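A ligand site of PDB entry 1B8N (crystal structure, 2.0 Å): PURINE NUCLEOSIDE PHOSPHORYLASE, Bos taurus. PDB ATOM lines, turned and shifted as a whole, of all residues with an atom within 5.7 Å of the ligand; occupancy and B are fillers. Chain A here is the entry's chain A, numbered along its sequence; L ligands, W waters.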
ATOM      1  N   SER A  33      20.718  -0.637 -20.684  1.00  0.00           N
ATOM      2  CA  SER A  33      19.462   0.050 -20.977  1.00  0.00           C
ATOM      3  C   SER A  33      19.392   0.679 -22.356  1.00  0.00           C
ATOM      4  O   SER A  33      20.294   1.417 -22.748  1.00  0.00           O
ATOM      5  CB  SER A  33      19.192   1.134 -19.942  1.00  0.00           C
ATOM      6  OG  SER A  33      18.899   0.554 -18.699  1.00  0.00           O
ATOM      7  N   VAL A  61      13.549  -4.269 -15.718  1.00  0.00           N
ATOM      8  CA  VAL A  61      13.684  -2.852 -16.003  1.00  0.00           C
ATOM      9  C   VAL A  61      13.277  -2.594 -17.442  1.00  0.00           C
ATOM     10  O   VAL A  61      13.591  -3.388 -18.337  1.00  0.00           O
ATOM     11  CB  VAL A  61      15.142  -2.391 -15.794  1.00  0.00           C
ATOM     12  CG1 VAL A  61      15.285  -0.902 -16.065  1.00  0.00           C
ATOM     13  CG2 VAL A  61      15.594  -2.740 -14.390  1.00  0.00           C
ATOM     14  N   HIS A  64      14.976  -3.579 -21.129  1.00  0.00           N
ATOM     15  CA  HIS A  64      15.675  -4.858 -20.974  1.00  0.00           C
ATOM     16  C   HIS A  64      14.718  -5.991 -21.376  1.00  0.00           C
ATOM     17  O   HIS A  64      13.805  -6.350 -20.630  1.00  0.00           O
ATOM     18  CB  HIS A  64      16.170  -5.032 -19.534  1.00  0.00           C
ATOM     19  CG  HIS A  64      17.200  -4.028 -19.116  1.00  0.00           C
ATOM     20  ND1 HIS A  64      16.895  -2.720 -18.823  1.00  0.00           N
ATOM     21  CD2 HIS A  64      18.547  -4.147 -18.953  1.00  0.00           C
ATOM     22  CE1 HIS A  64      18.001  -2.066 -18.505  1.00  0.00           C
ATOM     23  NE2 HIS A  64      19.011  -2.907 -18.573  1.00  0.00           N
ATOM     24  N   HIS A  86      20.170  -5.945 -12.165  1.00  0.00           N
ATOM     25  CA  HIS A  86      20.764  -4.932 -11.310  1.00  0.00           C
ATOM     26  C   HIS A  86      20.440  -5.211  -9.868  1.00  0.00           C
ATOM     27  O   HIS A  86      19.438  -5.840  -9.548  1.00  0.00           O
ATOM     28  CB  HIS A  86      20.204  -3.561 -11.671  1.00  0.00           C
ATOM     29  CG  HIS A  86      20.285  -3.218 -13.113  1.00  0.00           C
ATOM     30  ND1 HIS A  86      19.401  -3.720 -14.052  1.00  0.00           N
ATOM     31  CD2 HIS A  86      21.121  -2.393 -13.789  1.00  0.00           C
ATOM     32  CE1 HIS A  86      19.684  -3.213 -15.243  1.00  0.00           C
ATOM     33  NE2 HIS A  86      20.725  -2.401 -15.106  1.00  0.00           N
ATOM     34  N   TYR A  88      19.496  -2.964  -7.603  1.00  0.00           N
ATOM     35  CA  TYR A  88      18.279  -2.254  -7.173  1.00  0.00           C
ATOM     36  C   TYR A  88      16.974  -2.995  -7.454  1.00  0.00           C
ATOM     37  O   TYR A  88      15.933  -2.603  -6.955  1.00  0.00           O
ATOM     38  CB  TYR A  88      18.232  -0.824  -7.764  1.00  0.00           C
ATOM     39  CG  TYR A  88      18.246  -0.768  -9.290  1.00  0.00           C
ATOM     40  CD1 TYR A  88      17.147  -1.185 -10.025  1.00  0.00           C
ATOM     41  CD2 TYR A  88      19.363  -0.275  -9.990  1.00  0.00           C
ATOM     42  CE1 TYR A  88      17.133  -1.123 -11.413  1.00  0.00           C
ATOM     43  CE2 TYR A  88      19.370  -0.220 -11.382  1.00  0.00           C
ATOM     44  CZ  TYR A  88      18.239  -0.647 -12.079  1.00  0.00           C
ATOM     45  OH  TYR A  88      18.206  -0.617 -13.451  1.00  0.00           O
ATOM     46  N   ALA A 116      24.195   2.267 -20.026  1.00  0.00           N
ATOM     47  CA  ALA A 116      23.814   3.667 -20.206  1.00  0.00           C
ATOM     48  C   ALA A 116      24.303   4.296 -18.902  1.00  0.00           C
ATOM     49  O   ALA A 116      24.077   3.751 -17.807  1.00  0.00           O
ATOM     50  CB  ALA A 116      22.314   3.812 -20.328  1.00  0.00           C
ATOM     51  N   ALA A 117      25.039   5.392 -19.002  1.00  0.00           N
ATOM     52  CA  ALA A 117      25.575   6.060 -17.833  1.00  0.00           C
ATOM     53  C   ALA A 117      25.388   7.554 -17.934  1.00  0.00           C
ATOM     54  O   ALA A 117      25.303   8.103 -19.028  1.00  0.00           O
ATOM     55  CB  ALA A 117      27.041   5.734 -17.715  1.00  0.00           C
ATOM     56  N   GLY A 118      25.245   8.211 -16.799  1.00  0.00           N
ATOM     57  CA  GLY A 118      25.104   9.652 -16.812  1.00  0.00           C
ATOM     58  C   GLY A 118      26.533  10.169 -16.823  1.00  0.00           C
ATOM     59  O   GLY A 118      27.405   9.569 -16.174  1.00  0.00           O
ATOM     60  N   GLY A 119      26.794  11.229 -17.559  1.00  0.00           N
ATOM     61  CA  GLY A 119      28.145  11.766 -17.619  1.00  0.00           C
ATOM     62  C   GLY A 119      28.504  12.661 -16.453  1.00  0.00           C
ATOM     63  O   GLY A 119      27.685  13.486 -16.025  1.00  0.00           O
ATOM     64  N   TYR A 192      34.483   4.623 -14.793  1.00  0.00           N
ATOM     65  CA  TYR A 192      33.060   4.452 -14.513  1.00  0.00           C
ATOM     66  C   TYR A 192      32.885   4.132 -13.040  1.00  0.00           C
ATOM     67  O   TYR A 192      33.610   3.283 -12.492  1.00  0.00           O
ATOM     68  CB  TYR A 192      32.509   3.292 -15.362  1.00  0.00           C
ATOM     69  CG  TYR A 192      31.082   2.866 -15.067  1.00  0.00           C
ATOM     70  CD1 TYR A 192      30.006   3.394 -15.796  1.00  0.00           C
ATOM     71  CD2 TYR A 192      30.795   1.888 -14.099  1.00  0.00           C
ATOM     72  CE1 TYR A 192      28.714   2.951 -15.584  1.00  0.00           C
ATOM     73  CE2 TYR A 192      29.504   1.431 -13.882  1.00  0.00           C
ATOM     74  CZ  TYR A 192      28.468   1.974 -14.635  1.00  0.00           C
ATOM     75  OH  TYR A 192      27.187   1.530 -14.422  1.00  0.00           O
ATOM     76  N   LEU A 195      27.142   2.717  -8.365  1.00  0.00           N
ATOM     77  CA  LEU A 195      26.522   2.874  -7.058  1.00  0.00           C
ATOM     78  C   LEU A 195      25.217   2.089  -7.147  1.00  0.00           C
ATOM     79  O   LEU A 195      24.850   1.650  -8.235  1.00  0.00           O
ATOM     80  CB  LEU A 195      26.279   4.339  -6.691  1.00  0.00           C
ATOM     81  CG  LEU A 195      26.074   5.332  -7.831  1.00  0.00           C
ATOM     82  CD1 LEU A 195      24.830   4.930  -8.654  1.00  0.00           C
ATOM     83  CD2 LEU A 195      25.930   6.733  -7.222  1.00  0.00           C
ATOM     84  N   ASN A 199      17.337   5.439  -7.359  1.00  0.00           N
ATOM     85  CA  ASN A 199      17.155   6.877  -7.523  1.00  0.00           C
ATOM     86  C   ASN A 199      18.357   7.525  -8.208  1.00  0.00           C
ATOM     87  O   ASN A 199      19.471   6.994  -8.144  1.00  0.00           O
ATOM     88  CB  ASN A 199      16.909   7.550  -6.170  1.00  0.00           C
ATOM     89  CG  ASN A 199      18.103   7.493  -5.271  1.00  0.00           C
ATOM     90  OD1 ASN A 199      18.366   6.468  -4.630  1.00  0.00           O
ATOM     91  ND2 ASN A 199      18.883   8.567  -5.256  1.00  0.00           N
ATOM     92  N   PHE A 200      18.123   8.637  -8.881  1.00  0.00           N
ATOM     93  CA  PHE A 200      19.223   9.322  -9.540  1.00  0.00           C
ATOM     94  C   PHE A 200      19.930  10.189  -8.497  1.00  0.00           C
ATOM     95  O   PHE A 200      19.392  10.441  -7.431  1.00  0.00           O
ATOM     96  CB  PHE A 200      18.717  10.110 -10.753  1.00  0.00           C
ATOM     97  CG  PHE A 200      18.318   9.233 -11.935  1.00  0.00           C
ATOM     98  CD1 PHE A 200      19.291   8.582 -12.682  1.00  0.00           C
ATOM     99  CD2 PHE A 200      16.980   9.068 -12.290  1.00  0.00           C
ATOM    100  CE1 PHE A 200      18.944   7.780 -13.766  1.00  0.00           C
ATOM    101  CE2 PHE A 200      16.623   8.266 -13.374  1.00  0.00           C
ATOM    102  CZ  PHE A 200      17.605   7.625 -14.117  1.00  0.00           C
ATOM    103  N   GLU A 201      21.159  10.605  -8.817  1.00  0.00           N
ATOM    104  CA  GLU A 201      21.986  11.396  -7.899  1.00  0.00           C
ATOM    105  C   GLU A 201      21.455  12.771  -7.523  1.00  0.00           C
ATOM    106  O   GLU A 201      20.595  13.345  -8.208  1.00  0.00           O
ATOM    107  CB  GLU A 201      23.397  11.606  -8.498  1.00  0.00           C
ATOM    108  CG  GLU A 201      24.265  10.354  -8.683  1.00  0.00           C
ATOM    109  CD  GLU A 201      23.721   9.377  -9.731  1.00  0.00           C
ATOM    110  OE1 GLU A 201      23.455   9.737 -10.896  1.00  0.00           O
ATOM    111  OE2 GLU A 201      23.544   8.199  -9.368  1.00  0.00           O
ATOM    112  N   VAL A 217      28.718   7.538 -14.253  1.00  0.00           N
ATOM    113  CA  VAL A 217      28.116   6.799 -13.151  1.00  0.00           C
ATOM    114  C   VAL A 217      26.901   5.968 -13.576  1.00  0.00           C
ATOM    115  O   VAL A 217      26.072   6.414 -14.382  1.00  0.00           O
ATOM    116  CB  VAL A 217      27.702   7.792 -12.000  1.00  0.00           C
ATOM    117  CG1 VAL A 217      26.759   8.885 -12.542  1.00  0.00           C
ATOM    118  CG2 VAL A 217      27.028   7.032 -10.866  1.00  0.00           C
ATOM    119  N   GLY A 218      26.805   4.758 -13.035  1.00  0.00           N
ATOM    120  CA  GLY A 218      25.695   3.875 -13.325  1.00  0.00           C
ATOM    121  C   GLY A 218      25.384   2.956 -12.146  1.00  0.00           C
ATOM    122  O   GLY A 218      25.992   3.045 -11.072  1.00  0.00           O
ATOM    123  N   MET A 219      24.492   2.006 -12.371  1.00  0.00           N
ATOM    124  CA  MET A 219      24.088   1.085 -11.310  1.00  0.00           C
ATOM    125  C   MET A 219      24.295  -0.366 -11.749  1.00  0.00           C
ATOM    126  O   MET A 219      23.612  -1.265 -11.263  1.00  0.00           O
ATOM    127  CB  MET A 219      22.600   1.301 -10.978  1.00  0.00           C
ATOM    128  CG  MET A 219      22.198   2.759 -10.813  1.00  0.00           C
ATOM    129  SD  MET A 219      20.416   2.975 -10.775  1.00  0.00           S
ATOM    130  CE  MET A 219      20.255   4.728 -10.763  1.00  0.00           C
ATOM    131  N   SER A 220      25.262  -0.590 -12.626  1.00  0.00           N
ATOM    132  CA  SER A 220      25.520  -1.927 -13.128  1.00  0.00           C
ATOM    133  C   SER A 220      26.970  -2.072 -13.538  1.00  0.00           C
ATOM    134  O   SER A 220      27.855  -1.344 -13.079  1.00  0.00           O
ATOM    135  CB  SER A 220      24.664  -2.151 -14.362  1.00  0.00           C
ATOM    136  OG  SER A 220      25.205  -1.419 -15.459  1.00  0.00           O
ATOM    137  N   THR A 242      24.105   8.689 -21.716  1.00  0.00           N
ATOM    138  CA  THR A 242      22.689   8.968 -21.979  1.00  0.00           C
ATOM    139  C   THR A 242      22.132  10.274 -21.471  1.00  0.00           C
ATOM    140  O   THR A 242      21.094  10.720 -21.949  1.00  0.00           O
ATOM    141  CB  THR A 242      21.812   7.840 -21.485  1.00  0.00           C
ATOM    142  OG1 THR A 242      22.155   7.541 -20.126  1.00  0.00           O
ATOM    143  CG2 THR A 242      22.007   6.613 -22.361  1.00  0.00           C
ATOM    144  N   ASN A 243      22.813  10.904 -20.542  1.00  0.00           N
ATOM    145  CA  ASN A 243      22.373  12.163 -19.952  1.00  0.00           C
ATOM    146  C   ASN A 243      23.535  12.706 -19.149  1.00  0.00           C
ATOM    147  O   ASN A 243      24.468  11.977 -18.812  1.00  0.00           O
ATOM    148  CB  ASN A 243      21.196  11.911 -19.027  1.00  0.00           C
ATOM    149  CG  ASN A 243      21.518  10.846 -17.976  1.00  0.00           C
ATOM    150  OD1 ASN A 243      21.731   9.680 -18.313  1.00  0.00           O
ATOM    151  ND2 ASN A 243      21.585  11.252 -16.704  1.00  0.00           N
ATOM    152  N   VAL A 245      24.529  14.194 -15.676  1.00  0.00           N
ATOM    153  CA  VAL A 245      23.969  14.321 -14.348  1.00  0.00           C
ATOM    154  C   VAL A 245      23.983  15.806 -13.927  1.00  0.00           C
ATOM    155  O   VAL A 245      24.931  16.522 -14.226  1.00  0.00           O
ATOM    156  CB  VAL A 245      24.648  13.361 -13.285  1.00  0.00           C
ATOM    157  CG1 VAL A 245      25.162  12.096 -13.942  1.00  0.00           C
ATOM    158  CG2 VAL A 245      25.751  14.042 -12.582  1.00  0.00           C
ATOM    159  N   ALA A 255      17.212  13.919 -14.262  1.00  0.00           N
ATOM    160  CA  ALA A 255      17.524  12.657 -14.881  1.00  0.00           C
ATOM    161  C   ALA A 255      16.249  11.815 -14.942  1.00  0.00           C
ATOM    162  O   ALA A 255      15.405  11.881 -14.052  1.00  0.00           O
ATOM    163  CB  ALA A 255      18.602  11.940 -14.092  1.00  0.00           C
ATOM    164  N   ASN A 256      16.082  11.077 -16.042  1.00  0.00           N
ATOM    165  CA  ASN A 256      14.923  10.221 -16.195  1.00  0.00           C
ATOM    166  C   ASN A 256      15.160   9.060 -17.149  1.00  0.00           C
ATOM    167  O   ASN A 256      15.836   9.196 -18.189  1.00  0.00           O
ATOM    168  CB  ASN A 256      13.680  11.022 -16.598  1.00  0.00           C
ATOM    169  CG  ASN A 256      13.763  11.571 -18.001  1.00  0.00           C
ATOM    170  OD1 ASN A 256      13.160  11.028 -18.939  1.00  0.00           O
ATOM    171  ND2 ASN A 256      14.512  12.651 -18.154  1.00  0.00           N
ATOM    172  N   HIS A 257      14.601   7.915 -16.785  1.00  0.00           N
ATOM    173  CA  HIS A 257      14.770   6.704 -17.563  1.00  0.00           C
ATOM    174  C   HIS A 257      14.236   6.805 -18.976  1.00  0.00           C
ATOM    175  O   HIS A 257      14.726   6.147 -19.872  1.00  0.00           O
ATOM    176  CB  HIS A 257      14.112   5.539 -16.842  1.00  0.00           C
ATOM    177  CG  HIS A 257      14.597   4.213 -17.318  1.00  0.00           C
ATOM    178  ND1 HIS A 257      15.934   3.909 -17.409  1.00  0.00           N
ATOM    179  CD2 HIS A 257      13.931   3.116 -17.735  1.00  0.00           C
ATOM    180  CE1 HIS A 257      16.074   2.666 -17.845  1.00  0.00           C
ATOM    181  NE2 HIS A 257      14.878   2.163 -18.054  1.00  0.00           N
ATOM    182  N   VAL A 260      16.836   8.377 -21.119  1.00  0.00           N
ATOM    183  CA  VAL A 260      17.930   7.422 -21.197  1.00  0.00           C
ATOM    184  C   VAL A 260      17.681   6.400 -22.301  1.00  0.00           C
ATOM    185  O   VAL A 260      18.547   6.136 -23.135  1.00  0.00           O
ATOM    186  CB  VAL A 260      18.144   6.712 -19.820  1.00  0.00           C
ATOM    187  CG1 VAL A 260      19.088   5.484 -19.956  1.00  0.00           C
ATOM    188  CG2 VAL A 260      18.699   7.722 -18.811  1.00  0.00           C
HETATM  189  O1  LIG L   1      18.077   4.989 -16.512  1.00  0.00           O
HETATM  190  C1  LIG L   1      18.614   4.301 -15.381  1.00  0.00           C
HETATM  191  C2  LIG L   1      19.329   2.943 -15.639  1.00  0.00           C
HETATM  192  N1  LIG L   1      20.364   3.322 -16.606  1.00  0.00           N
HETATM  193  C3  LIG L   1      20.133   2.285 -14.470  1.00  0.00           C
HETATM  194  O2  LIG L   1      20.353   0.853 -14.618  1.00  0.00           O
HETATM  195  C4  LIG L   1      21.528   2.993 -14.507  1.00  0.00           C
HETATM  196  O3  LIG L   1      22.608   2.066 -14.357  1.00  0.00           O
HETATM  197  C5  LIG L   1      21.608   3.649 -15.900  1.00  0.00           C
HETATM  198  C6  LIG L   1      21.759   5.268 -15.854  1.00  0.00           C
HETATM  199  C7  LIG L   1      21.512   6.107 -16.872  1.00  0.00           C
HETATM  200  N2  LIG L   1      21.770   7.455 -16.444  1.00  0.00           N
HETATM  201  C8  LIG L   1      22.168   7.333 -15.093  1.00  0.00           C
HETATM  202  C9  LIG L   1      22.557   8.438 -14.200  1.00  0.00           C
HETATM  203  O4  LIG L   1      22.543   9.666 -14.398  1.00  0.00           O
HETATM  204  N3  LIG L   1      22.894   7.904 -12.975  1.00  0.00           N
HETATM  205  N4  LIG L   1      23.425   6.195 -11.393  1.00  0.00           N
HETATM  206  C10 LIG L   1      22.903   6.553 -12.627  1.00  0.00           C
HETATM  207  N5  LIG L   1      22.548   5.619 -13.498  1.00  0.00           N
HETATM  208  C11 LIG L   1      22.193   6.054 -14.707  1.00  0.00           C
HETATM  209  O   HOH W   1      25.184   2.096 -15.982  1.00  0.00           O
HETATM  210  O   HOH W   2      21.536  11.321 -12.499  1.00  0.00           O
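The backbone NH of Met 219 is in hydrogen-bond range of an oxygen (O3) of the ligand, 2.7 Å away.
ND1 of His 257 sits at hydrogen-bond distance from O1 of the ligand (2.6 Å).
The side-chain amide oxygen (OD1) of Asn 243 sits at hydrogen-bond distance from a nitrogen (N2) of the ligand, 2.9 Å away.
The side-chain carboxylate (OE1) of Glu 201 sits at hydrogen-bond distance from a nitrogen (N3) of the ligand (2.8 Å).
OH of Tyr 88 is in hydrogen-bond range of O2 of the ligand, 2.9 Å away.
NE2 of His 86 sits at hydrogen-bond distance from O2 of the ligand (3.3 Å).
Ser 33 touches the ligand (OG to N1, 3.8 Å).
Ala 116 touches the ligand (O to C5, 3.1 Å).
C of Ala 117 touches N2 of the ligand (3.9 Å).
CA of Gly 118 touches O4 of the ligand, 3.5 Å away.
CD1 of Leu 195 touches N4 of the ligand (3.3 Å).
Phe 200 touches the ligand (CE1 to C8, 3.5 Å).
O of Val 217 touches C10 of the ligand (3.6 Å).
CA of Gly 218 touches N5 of the ligand, 3.6 Å away.
Thr 242 touches the ligand.
Val 245 touches the ligand.
Val 260 touches the ligand.
Hydrophobic or aromatic side chains within 4 Å of the ligand: His 86, Tyr 88, Leu 195, Phe 200, Val 217, Met 219, Val 245, His 257 and Val 260.
17 residues have an atom within 4 Å of the ligand: Ser 33, His 86, Tyr 88, Ala 116, Ala 117, Gly 118, Leu 195, Phe 200, Glu 201, Val 217, Gly 218, Met 219, Thr 242, Asn 243, Val 245, His 257 and Val 260.
N of Leu 195 lies within hydrogen-bond range of O of Gly 218.
A ring nitrogen (ND1) of His 86 lies close to the side-chain hydroxyl (OH) of Tyr 88, at 3.4 Å.
The backbone carbonyl oxygen (O) of Gly 118 is in hydrogen-bond range of the backbone NH (N) of Val 217.
N of Met 219 is in hydrogen-bond range of OH of Tyr 192 (3.4 Å).
N of Thr 242 sits at hydrogen-bond distance from O of Ala 117.
The backbone carbonyl oxygen (O) of Asn 243 is in hydrogen-bond range of the backbone NH (N) of Gly 119 (2.7 Å).
N of Val 245 is in hydrogen-bond range of O of Gly 119, 3.3 Å away.
A ring nitrogen (NE2) of His 64 lies close to the side-chain hydroxyl (OG) of Ser 33, at 3.5 Å.
Water W2 lies within hydrogen-bond range of an oxygen (O4) of the ligand (2.7 Å) and the side-chain carboxylate of Glu 201 (3.0 Å).
Water W1 lies within hydrogen-bond range of the side-chain hydroxyl (OH) of Tyr 192, the backbone carbonyl oxygen (O) of Ala 116 and an oxygen (O3) of the ligand.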
